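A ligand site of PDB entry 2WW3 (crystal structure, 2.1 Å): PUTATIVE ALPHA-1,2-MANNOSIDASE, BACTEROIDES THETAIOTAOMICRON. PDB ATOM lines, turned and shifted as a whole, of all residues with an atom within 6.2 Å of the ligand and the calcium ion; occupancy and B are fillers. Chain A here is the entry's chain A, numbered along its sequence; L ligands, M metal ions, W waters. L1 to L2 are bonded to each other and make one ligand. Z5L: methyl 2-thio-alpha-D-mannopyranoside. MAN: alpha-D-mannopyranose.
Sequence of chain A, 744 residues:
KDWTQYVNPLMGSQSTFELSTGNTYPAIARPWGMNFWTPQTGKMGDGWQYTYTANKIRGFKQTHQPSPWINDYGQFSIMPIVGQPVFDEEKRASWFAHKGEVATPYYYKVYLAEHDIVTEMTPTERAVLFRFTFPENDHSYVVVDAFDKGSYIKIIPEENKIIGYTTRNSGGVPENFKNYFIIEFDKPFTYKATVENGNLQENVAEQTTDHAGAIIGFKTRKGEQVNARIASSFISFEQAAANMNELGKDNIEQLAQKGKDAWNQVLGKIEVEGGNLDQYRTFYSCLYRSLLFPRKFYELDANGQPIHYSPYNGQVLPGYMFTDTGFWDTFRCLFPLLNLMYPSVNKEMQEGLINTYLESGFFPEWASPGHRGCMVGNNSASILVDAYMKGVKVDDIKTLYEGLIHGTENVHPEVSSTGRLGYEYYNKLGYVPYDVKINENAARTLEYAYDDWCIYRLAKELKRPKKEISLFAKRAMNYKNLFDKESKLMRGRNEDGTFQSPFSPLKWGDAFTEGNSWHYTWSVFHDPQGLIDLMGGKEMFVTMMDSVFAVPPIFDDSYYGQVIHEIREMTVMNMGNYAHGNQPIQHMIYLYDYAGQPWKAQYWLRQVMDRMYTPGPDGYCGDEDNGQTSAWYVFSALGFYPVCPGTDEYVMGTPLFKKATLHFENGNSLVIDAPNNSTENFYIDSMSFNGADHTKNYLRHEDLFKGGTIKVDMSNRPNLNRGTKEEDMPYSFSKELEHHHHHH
The side-chain carboxylate of Asp 329 sits at hydrogen-bond distance from an oxygen (O4) of MAN L2 (2.6 Å).
The side-chain hydroxyl of Ser 67 sits at hydrogen-bond distance from an oxygen (O6) of MAN L2 (2.6 Å).
The indole nitrogen (NE1) of Trp 366 is in hydrogen-bond range of an oxygen (O4) of MAN L2 (3.2 Å).
NE2 of His 565 is in hydrogen-bond range of O3 of Z5L L1 (2.8 Å).
OD2 of Asp 623 lies close to O2 of MAN L2 (2.9 Å).
The indole nitrogen (NE1) of Trp 69 sits close to an oxygen (O3) of Z5L L1 (3.4 Å).
The side-chain carboxylate of Glu 566 lies within hydrogen-bond range of an oxygen (O3) of Z5L L1 (2.6 Å).
Water W2 lies within hydrogen-bond range of O of Asp 623 (3.3 Å) and NE2 of Gln 583 (3.4 Å).
The calcium ion is bound by the side-chain carboxylate (OD2) of Asp 625 (2.0 Å), water W1 (2.1 Å), an oxygen (O3) of MAN L2 (2.1 Å), the side-chain amide oxygen (OE1) of Gln 583 (2.2 Å), water W2 (2.3 Å) and an oxygen (O2) of MAN L2 (2.7 Å).
N of Ile 70 lies within hydrogen-bond range of OG of Ser 67, 3.2 Å away.
A ring nitrogen (NE2) of His 565 sits at hydrogen-bond distance from the side-chain carboxylate of Glu 566, at 3.3 Å.
The side-chain carboxylate (OD1) of Asp 623 sits at hydrogen-bond distance from the side-chain amide nitrogen (ND2) of Asn 23, 2.7 Å away.
The side-chain carboxylate (OD2) of Asp 623 is in hydrogen-bond range of the indole nitrogen (NE1) of Trp 69 (2.8 Å).
The side-chain carboxylate (OE2) of Glu 566 lies close to the side-chain carboxylate (OE2) of Glu 514 (2.4 Å).
The side-chain amide oxygen (OE1) of Gln 583 lies close to the side-chain carboxylate (OD2) of Asp 329.
The backbone NH (N) of Trp 69 lies close to the side-chain hydroxyl (OG) of Ser 67 (3.5 Å).
The side-chain amide oxygen of Asn 582 lies close to the backbone carbonyl oxygen of Glu 514, 2.7 Å away.
OD2 of Asp 329 touches the calcium ion, at 3.8 Å.
Three residues have an atom within 4 Å of the calcium ion: Asp 329, Gln 583 and Asp 625.
Along chain A the residues within 4 Å of the calcium ion span positions 329 to 625.
A sulfur (S2) of Z5L L1 sits close to the side-chain carboxylate (OE1) of Glu 514 (3.6 Å).
Ile 70 touches the ligand.
Trp 328 touches the ligand.
Cys 374 touches the ligand.
Met 375 touches the ligand.
CB of Ile 564 touches O4 of Z5L L1, at 3.8 Å.
Within 4 Å of the ligand: Ser 67, Trp 69, Ile 70, Trp 328, Asp 329, Trp 366, Cys 374, Met 375, Glu 514, Ile 564, His 565, Glu 566, Gln 583, Asp 623 and Asp 625.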
ATOM      1  N   ASN A  23      -2.723  -0.564 -11.597  1.00  0.00           N
ATOM      2  CA  ASN A  23      -3.303   0.422 -10.688  1.00  0.00           C
ATOM      3  C   ASN A  23      -2.287   1.464 -10.196  1.00  0.00           C
ATOM      4  O   ASN A  23      -2.182   1.759  -9.000  1.00  0.00           O
ATOM      5  CB  ASN A  23      -4.036  -0.267  -9.530  1.00  0.00           C
ATOM      6  CG  ASN A  23      -5.461  -0.652  -9.898  1.00  0.00           C
ATOM      7  OD1 ASN A  23      -6.068  -0.047 -10.803  1.00  0.00           O
ATOM      8  ND2 ASN A  23      -6.001  -1.640  -9.189  1.00  0.00           N
ATOM      9  N   PRO A  66      -0.414   5.164  -2.001  1.00  0.00           N
ATOM     10  CA  PRO A  66       0.261   3.927  -2.388  1.00  0.00           C
ATOM     11  C   PRO A  66      -0.595   3.010  -3.247  1.00  0.00           C
ATOM     12  O   PRO A  66      -0.034   2.150  -3.925  1.00  0.00           O
ATOM     13  CB  PRO A  66       0.531   3.237  -1.044  1.00  0.00           C
ATOM     14  CG  PRO A  66      -0.639   3.666  -0.202  1.00  0.00           C
ATOM     15  CD  PRO A  66      -0.871   5.119  -0.598  1.00  0.00           C
ATOM     16  N   SER A  67      -1.932   3.146  -3.207  1.00  0.00           N
ATOM     17  CA  SER A  67      -2.801   2.336  -4.081  1.00  0.00           C
ATOM     18  C   SER A  67      -4.231   2.852  -4.055  1.00  0.00           C
ATOM     19  O   SER A  67      -4.570   3.598  -3.169  1.00  0.00           O
ATOM     20  CB  SER A  67      -2.786   0.853  -3.710  1.00  0.00           C
ATOM     21  OG  SER A  67      -3.529   0.638  -2.519  1.00  0.00           O
ATOM     22  N   PRO A  68      -5.038   2.472  -5.055  1.00  0.00           N
ATOM     23  CA  PRO A  68      -6.395   3.012  -5.108  1.00  0.00           C
ATOM     24  C   PRO A  68      -7.227   2.432  -3.983  1.00  0.00           C
ATOM     25  O   PRO A  68      -8.204   3.045  -3.559  1.00  0.00           O
ATOM     26  CB  PRO A  68      -6.915   2.552  -6.477  1.00  0.00           C
ATOM     27  CG  PRO A  68      -6.070   1.365  -6.860  1.00  0.00           C
ATOM     28  CD  PRO A  68      -4.749   1.511  -6.142  1.00  0.00           C
ATOM     29  N   TRP A  69      -6.828   1.265  -3.474  1.00  0.00           N
ATOM     30  CA  TRP A  69      -7.539   0.641  -2.364  1.00  0.00           C
ATOM     31  C   TRP A  69      -7.303   1.376  -1.053  1.00  0.00           C
ATOM     32  O   TRP A  69      -8.235   1.652  -0.308  1.00  0.00           O
ATOM     33  CB  TRP A  69      -7.136  -0.842  -2.238  1.00  0.00           C
ATOM     34  CG  TRP A  69      -7.082  -1.460  -3.590  1.00  0.00           C
ATOM     35  CD1 TRP A  69      -5.962  -1.787  -4.311  1.00  0.00           C
ATOM     36  CD2 TRP A  69      -8.209  -1.753  -4.428  1.00  0.00           C
ATOM     37  NE1 TRP A  69      -6.338  -2.294  -5.545  1.00  0.00           N
ATOM     38  CE2 TRP A  69      -7.703  -2.273  -5.630  1.00  0.00           C
ATOM     39  CE3 TRP A  69      -9.589  -1.622  -4.268  1.00  0.00           C
ATOM     40  CZ2 TRP A  69      -8.536  -2.665  -6.666  1.00  0.00           C
ATOM     41  CZ3 TRP A  69     -10.411  -2.023  -5.284  1.00  0.00           C
ATOM     42  CH2 TRP A  69      -9.877  -2.541  -6.476  1.00  0.00           C
ATOM     43  N   ILE A  70      -6.040   1.688  -0.778  1.00  0.00           N
ATOM     44  CA  ILE A  70      -5.668   2.396   0.441  1.00  0.00           C
ATOM     45  C   ILE A  70      -6.050   3.870   0.345  1.00  0.00           C
ATOM     46  O   ILE A  70      -6.456   4.483   1.334  1.00  0.00           O
ATOM     47  CB  ILE A  70      -4.168   2.257   0.650  1.00  0.00           C
ATOM     48  CG1 ILE A  70      -3.800   0.794   0.933  1.00  0.00           C
ATOM     49  CG2 ILE A  70      -3.711   3.174   1.746  1.00  0.00           C
ATOM     50  CD1 ILE A  70      -4.285   0.300   2.305  1.00  0.00           C
ATOM     51  N   GLY A 326       2.987  -1.725   2.279  1.00  0.00           N
ATOM     52  CA  GLY A 326       2.489  -2.860   3.045  1.00  0.00           C
ATOM     53  C   GLY A 326       3.458  -4.031   2.960  1.00  0.00           C
ATOM     54  O   GLY A 326       3.702  -4.557   1.858  1.00  0.00           O
ATOM     55  N   TRP A 328       3.241  -7.078   3.604  1.00  0.00           N
ATOM     56  CA  TRP A 328       2.644  -8.269   2.992  1.00  0.00           C
ATOM     57  C   TRP A 328       2.976  -8.309   1.497  1.00  0.00           C
ATOM     58  O   TRP A 328       3.173  -9.389   0.950  1.00  0.00           O
ATOM     59  CB  TRP A 328       1.124  -8.306   3.200  1.00  0.00           C
ATOM     60  CG  TRP A 328       0.467  -9.580   2.640  1.00  0.00           C
ATOM     61  CD1 TRP A 328       0.342 -10.758   3.270  1.00  0.00           C
ATOM     62  CD2 TRP A 328      -0.111  -9.753   1.347  1.00  0.00           C
ATOM     63  NE1 TRP A 328      -0.309 -11.671   2.461  1.00  0.00           N
ATOM     64  CE2 TRP A 328      -0.588 -11.080   1.273  1.00  0.00           C
ATOM     65  CE3 TRP A 328      -0.274  -8.926   0.233  1.00  0.00           C
ATOM     66  CZ2 TRP A 328      -1.212 -11.599   0.133  1.00  0.00           C
ATOM     67  CZ3 TRP A 328      -0.917  -9.441  -0.894  1.00  0.00           C
ATOM     68  CH2 TRP A 328      -1.367 -10.770  -0.934  1.00  0.00           C
ATOM     69  N   ASP A 329       3.044  -7.142   0.858  1.00  0.00           N
ATOM     70  CA  ASP A 329       3.573  -7.066  -0.520  1.00  0.00           C
ATOM     71  C   ASP A 329       5.114  -7.095  -0.530  1.00  0.00           C
ATOM     72  O   ASP A 329       5.743  -7.935  -1.202  1.00  0.00           O
ATOM     73  CB  ASP A 329       3.115  -5.776  -1.248  1.00  0.00           C
ATOM     74  CG  ASP A 329       1.586  -5.653  -1.353  1.00  0.00           C
ATOM     75  OD1 ASP A 329       1.031  -4.580  -0.993  1.00  0.00           O
ATOM     76  OD2 ASP A 329       0.937  -6.628  -1.783  1.00  0.00           O
ATOM     77  N   TRP A 366       0.974  -2.764   7.367  1.00  0.00           N
ATOM     78  CA  TRP A 366       0.575  -1.817   6.334  1.00  0.00           C
ATOM     79  C   TRP A 366       0.520  -0.448   7.013  1.00  0.00           C
ATOM     80  O   TRP A 366      -0.155  -0.287   8.047  1.00  0.00           O
ATOM     81  CB  TRP A 366      -0.799  -2.150   5.757  1.00  0.00           C
ATOM     82  CG  TRP A 366      -0.775  -2.340   4.269  1.00  0.00           C
ATOM     83  CD1 TRP A 366      -1.056  -3.502   3.593  1.00  0.00           C
ATOM     84  CD2 TRP A 366      -0.440  -1.368   3.261  1.00  0.00           C
ATOM     85  NE1 TRP A 366      -0.921  -3.313   2.244  1.00  0.00           N
ATOM     86  CE2 TRP A 366      -0.553  -2.013   2.003  1.00  0.00           C
ATOM     87  CE3 TRP A 366      -0.066  -0.023   3.294  1.00  0.00           C
ATOM     88  CZ2 TRP A 366      -0.296  -1.360   0.804  1.00  0.00           C
ATOM     89  CZ3 TRP A 366       0.186   0.623   2.090  1.00  0.00           C
ATOM     90  CH2 TRP A 366       0.072  -0.048   0.866  1.00  0.00           C
ATOM     91  N   CYS A 374      -5.115  -3.723   6.682  1.00  0.00           N
ATOM     92  CA  CYS A 374      -5.055  -4.269   5.323  1.00  0.00           C
ATOM     93  C   CYS A 374      -4.139  -5.470   5.268  1.00  0.00           C
ATOM     94  O   CYS A 374      -3.042  -5.456   5.857  1.00  0.00           O
ATOM     95  CB  CYS A 374      -4.538  -3.207   4.350  1.00  0.00           C
ATOM     96  SG  CYS A 374      -4.853  -3.602   2.613  1.00  0.00           S
ATOM     97  N   MET A 375      -4.573  -6.498   4.559  1.00  0.00           N
ATOM     98  CA  MET A 375      -3.803  -7.726   4.393  1.00  0.00           C
ATOM     99  C   MET A 375      -3.512  -8.440   5.710  1.00  0.00           C
ATOM    100  O   MET A 375      -4.213  -8.202   6.687  1.00  0.00           O
ATOM    101  CB  MET A 375      -2.539  -7.496   3.548  1.00  0.00           C
ATOM    102  CG  MET A 375      -2.859  -6.738   2.256  1.00  0.00           C
ATOM    103  SD  MET A 375      -4.267  -7.479   1.376  1.00  0.00           S
ATOM    104  CE  MET A 375      -3.586  -9.040   1.008  1.00  0.00           C
ATOM    105  N   GLU A 514      -6.313 -13.202  -0.946  1.00  0.00           N
ATOM    106  CA  GLU A 514      -6.005 -12.830  -2.314  1.00  0.00           C
ATOM    107  C   GLU A 514      -5.735 -14.019  -3.201  1.00  0.00           C
ATOM    108  O   GLU A 514      -4.983 -13.890  -4.155  1.00  0.00           O
ATOM    109  CB  GLU A 514      -4.735 -11.947  -2.376  1.00  0.00           C
ATOM    110  CG  GLU A 514      -4.938 -10.520  -1.805  1.00  0.00           C
ATOM    111  CD  GLU A 514      -5.735  -9.613  -2.738  1.00  0.00           C
ATOM    112  OE1 GLU A 514      -6.946  -9.460  -2.516  1.00  0.00           O
ATOM    113  OE2 GLU A 514      -5.158  -9.082  -3.716  1.00  0.00           O
ATOM    114  N   TYR A 560     -16.218 -13.424  -1.590  1.00  0.00           N
ATOM    115  CA  TYR A 560     -16.252 -12.008  -1.950  1.00  0.00           C
ATOM    116  C   TYR A 560     -17.638 -11.547  -2.420  1.00  0.00           C
ATOM    117  O   TYR A 560     -17.991 -10.377  -2.241  1.00  0.00           O
ATOM    118  CB  TYR A 560     -15.211 -11.698  -3.013  1.00  0.00           C
ATOM    119  CG  TYR A 560     -13.817 -12.088  -2.587  1.00  0.00           C
ATOM    120  CD1 TYR A 560     -13.044 -11.217  -1.817  1.00  0.00           C
ATOM    121  CD2 TYR A 560     -13.272 -13.320  -2.936  1.00  0.00           C
ATOM    122  CE1 TYR A 560     -11.767 -11.564  -1.414  1.00  0.00           C
ATOM    123  CE2 TYR A 560     -11.990 -13.675  -2.528  1.00  0.00           C
ATOM    124  CZ  TYR A 560     -11.246 -12.790  -1.767  1.00  0.00           C
ATOM    125  OH  TYR A 560      -9.972 -13.110  -1.360  1.00  0.00           O
ATOM    126  N   ILE A 564     -13.869 -10.403  -7.928  1.00  0.00           N
ATOM    127  CA  ILE A 564     -12.912  -9.315  -7.722  1.00  0.00           C
ATOM    128  C   ILE A 564     -11.862  -9.385  -8.825  1.00  0.00           C
ATOM    129  O   ILE A 564     -11.584 -10.443  -9.381  1.00  0.00           O
ATOM    130  CB  ILE A 564     -12.259  -9.369  -6.334  1.00  0.00           C
ATOM    131  CG1 ILE A 564     -11.592 -10.734  -6.116  1.00  0.00           C
ATOM    132  CG2 ILE A 564     -13.315  -9.124  -5.266  1.00  0.00           C
ATOM    133  CD1 ILE A 564     -10.865 -10.832  -4.833  1.00  0.00           C
ATOM    134  N   HIS A 565     -11.272  -8.248  -9.153  1.00  0.00           N
ATOM    135  CA  HIS A 565     -10.354  -8.185 -10.271  1.00  0.00           C
ATOM    136  C   HIS A 565      -9.161  -9.187 -10.181  1.00  0.00           C
ATOM    137  O   HIS A 565      -8.703  -9.698 -11.199  1.00  0.00           O
ATOM    138  CB  HIS A 565      -9.889  -6.724 -10.416  1.00  0.00           C
ATOM    139  CG  HIS A 565      -9.058  -6.260  -9.263  1.00  0.00           C
ATOM    140  ND1 HIS A 565      -7.681  -6.250  -9.306  1.00  0.00           N
ATOM    141  CD2 HIS A 565      -9.412  -5.861  -8.027  1.00  0.00           C
ATOM    142  CE1 HIS A 565      -7.205  -5.847  -8.141  1.00  0.00           C
ATOM    143  NE2 HIS A 565      -8.243  -5.595  -7.343  1.00  0.00           N
ATOM    144  N   GLU A 566      -8.659  -9.514  -8.995  1.00  0.00           N
ATOM    145  CA  GLU A 566      -7.619 -10.557  -8.919  1.00  0.00           C
ATOM    146  C   GLU A 566      -8.081 -11.875  -9.564  1.00  0.00           C
ATOM    147  O   GLU A 566      -7.325 -12.544 -10.255  1.00  0.00           O
ATOM    148  CB  GLU A 566      -7.147 -10.797  -7.479  1.00  0.00           C
ATOM    149  CG  GLU A 566      -6.414  -9.607  -6.823  1.00  0.00           C
ATOM    150  CD  GLU A 566      -7.326  -8.673  -6.011  1.00  0.00           C
ATOM    151  OE1 GLU A 566      -8.552  -8.661  -6.270  1.00  0.00           O
ATOM    152  OE2 GLU A 566      -6.811  -7.962  -5.116  1.00  0.00           O
ATOM    153  N   GLY A 581       0.187 -11.782 -10.722  1.00  0.00           N
ATOM    154  CA  GLY A 581      -0.124 -10.621  -9.874  1.00  0.00           C
ATOM    155  C   GLY A 581      -0.370 -10.977  -8.414  1.00  0.00           C
ATOM    156  O   GLY A 581      -0.335 -10.120  -7.528  1.00  0.00           O
ATOM    157  N   ASN A 582      -0.647 -12.255  -8.172  1.00  0.00           N
ATOM    158  CA  ASN A 582      -0.835 -12.791  -6.831  1.00  0.00           C
ATOM    159  C   ASN A 582       0.482 -12.883  -6.045  1.00  0.00           C
ATOM    160  O   ASN A 582       1.309 -13.777  -6.321  1.00  0.00           O
ATOM    161  CB  ASN A 582      -1.400 -14.202  -6.979  1.00  0.00           C
ATOM    162  CG  ASN A 582      -2.242 -14.624  -5.804  1.00  0.00           C
ATOM    163  OD1 ASN A 582      -3.386 -15.060  -5.969  1.00  0.00           O
ATOM    164  ND2 ASN A 582      -1.682 -14.503  -4.614  1.00  0.00           N
ATOM    165  N   GLN A 583       0.689 -11.992  -5.079  1.00  0.00           N
ATOM    166  CA  GLN A 583       1.977 -11.934  -4.366  1.00  0.00           C
ATOM    167  C   GLN A 583       2.451 -13.257  -3.761  1.00  0.00           C
ATOM    168  O   GLN A 583       3.616 -13.595  -3.849  1.00  0.00           O
ATOM    169  CB  GLN A 583       1.956 -10.851  -3.272  1.00  0.00           C
ATOM    170  CG  GLN A 583       2.570  -9.528  -3.751  1.00  0.00           C
ATOM    171  CD  GLN A 583       1.592  -8.648  -4.538  1.00  0.00           C
ATOM    172  OE1 GLN A 583       0.394  -8.712  -4.348  1.00  0.00           O
ATOM    173  NE2 GLN A 583       2.126  -7.810  -5.424  1.00  0.00           N
ATOM    174  N   ASP A 623      -2.058  -5.720  -9.797  1.00  0.00           N
ATOM    175  CA  ASP A 623      -1.627  -4.546  -9.049  1.00  0.00           C
ATOM    176  C   ASP A 623      -0.115  -4.483  -8.908  1.00  0.00           C
ATOM    177  O   ASP A 623       0.534  -5.495  -8.661  1.00  0.00           O
ATOM    178  CB  ASP A 623      -2.272  -4.477  -7.659  1.00  0.00           C
ATOM    179  CG  ASP A 623      -3.684  -3.917  -7.687  1.00  0.00           C
ATOM    180  OD1 ASP A 623      -4.231  -3.620  -8.773  1.00  0.00           O
ATOM    181  OD2 ASP A 623      -4.274  -3.792  -6.592  1.00  0.00           O
ATOM    182  N   GLU A 624       0.452  -3.299  -9.049  1.00  0.00           N
ATOM    183  CA  GLU A 624       1.911  -3.177  -8.953  1.00  0.00           C
ATOM    184  C   GLU A 624       2.431  -3.301  -7.504  1.00  0.00           C
ATOM    185  O   GLU A 624       3.478  -3.904  -7.271  1.00  0.00           O
ATOM    186  CB  GLU A 624       2.368  -1.861  -9.599  1.00  0.00           C
ATOM    187  CG  GLU A 624       3.845  -1.798  -9.877  1.00  0.00           C
ATOM    188  CD  GLU A 624       4.650  -1.432  -8.648  1.00  0.00           C
ATOM    189  OE1 GLU A 624       4.056  -0.780  -7.764  1.00  0.00           O
ATOM    190  OE2 GLU A 624       5.863  -1.793  -8.584  1.00  0.00           O
ATOM    191  N   ASP A 625       1.671  -2.720  -6.560  1.00  0.00           N
ATOM    192  CA  ASP A 625       1.922  -2.818  -5.103  1.00  0.00           C
ATOM    193  C   ASP A 625       3.244  -2.264  -4.615  1.00  0.00           C
ATOM    194  O   ASP A 625       4.055  -2.976  -4.022  1.00  0.00           O
ATOM    195  CB  ASP A 625       1.739  -4.256  -4.609  1.00  0.00           C
ATOM    196  CG  ASP A 625       0.329  -4.754  -4.806  1.00  0.00           C
ATOM    197  OD1 ASP A 625      -0.634  -3.998  -4.486  1.00  0.00           O
ATOM    198  OD2 ASP A 625       0.186  -5.905  -5.303  1.00  0.00           O
ATOM    199  N   ASN A 626       3.470  -0.987  -4.884  1.00  0.00           N
ATOM    200  CA  ASN A 626       4.538  -0.218  -4.235  1.00  0.00           C
ATOM    201  C   ASN A 626       5.924  -0.790  -4.411  1.00  0.00           C
ATOM    202  O   ASN A 626       6.788  -0.653  -3.543  1.00  0.00           O
ATOM    203  CB  ASN A 626       4.204  -0.061  -2.757  1.00  0.00           C
ATOM    204  CG  ASN A 626       2.793   0.380  -2.575  1.00  0.00           C
ATOM    205  OD1 ASN A 626       1.936  -0.415  -2.201  1.00  0.00           O
ATOM    206  ND2 ASN A 626       2.494   1.611  -3.016  1.00  0.00           N
ATOM    207  N   THR A 629       5.728  -5.982  -7.397  1.00  0.00           N
ATOM    208  CA  THR A 629       5.617  -6.612  -8.715  1.00  0.00           C
ATOM    209  C   THR A 629       6.667  -6.102  -9.705  1.00  0.00           C
ATOM    210  O   THR A 629       7.073  -6.826 -10.663  1.00  0.00           O
ATOM    211  CB  THR A 629       4.210  -6.456  -9.275  1.00  0.00           C
ATOM    212  OG1 THR A 629       3.267  -6.960  -8.315  1.00  0.00           O
ATOM    213  CG2 THR A 629       4.045  -7.214 -10.584  1.00  0.00           C
HETATM  214  S2  Z5L L   1      -6.158  -5.933  -2.033  1.00  0.00           S
HETATM  215  C2  Z5L L   1      -7.558  -4.865  -2.394  1.00  0.00           C
HETATM  216  C1  Z5L L   1      -8.523  -4.768  -1.217  1.00  0.00           C
HETATM  217  O1  Z5L L   1      -9.414  -3.653  -1.431  1.00  0.00           O
HETATM  218  C1M Z5L L   1     -10.349  -3.461  -0.367  1.00  0.00           C
HETATM  219  O5  Z5L L   1      -9.242  -6.000  -1.078  1.00  0.00           O
HETATM  220  C3  Z5L L   1      -8.305  -5.271  -3.662  1.00  0.00           C
HETATM  221  O3  Z5L L   1      -7.364  -5.478  -4.711  1.00  0.00           O
HETATM  222  C4  Z5L L   1      -9.121  -6.546  -3.415  1.00  0.00           C
HETATM  223  O4  Z5L L   1      -9.934  -6.905  -4.532  1.00  0.00           O
HETATM  224  C5  Z5L L   1     -10.032  -6.348  -2.212  1.00  0.00           C
HETATM  225  C6  Z5L L   1     -10.783  -7.656  -1.945  1.00  0.00           C
HETATM  226  O6  Z5L L   1     -11.176  -7.699  -0.567  1.00  0.00           O
HETATM  227  C1  MAN L   2      -4.924  -5.076  -2.987  1.00  0.00           C
HETATM  228  C2  MAN L   2      -3.759  -6.002  -3.346  1.00  0.00           C
HETATM  229  C3  MAN L   2      -2.713  -6.103  -2.222  1.00  0.00           C
HETATM  230  C4  MAN L   2      -2.413  -4.716  -1.668  1.00  0.00           C
HETATM  231  C5  MAN L   2      -3.688  -4.051  -1.189  1.00  0.00           C
HETATM  232  C6  MAN L   2      -3.354  -2.690  -0.574  1.00  0.00           C
HETATM  233  O2  MAN L   2      -3.192  -5.459  -4.537  1.00  0.00           O
HETATM  234  O3  MAN L   2      -1.507  -6.668  -2.750  1.00  0.00           O
HETATM  235  O4  MAN L   2      -1.533  -4.758  -0.563  1.00  0.00           O
HETATM  236  O5  MAN L   2      -4.519  -3.857  -2.329  1.00  0.00           O
HETATM  237  O6  MAN L   2      -3.018  -1.732  -1.584  1.00  0.00           O
HETATM  238 CA    CA M   1      -1.239  -7.275  -4.786  1.00  0.00          CA
HETATM  239  O   HOH W   1      -2.441  -8.959  -4.969  1.00  0.00           O
HETATM  240  O   HOH W   2      -0.942  -7.966  -6.984  1.00  0.00           O
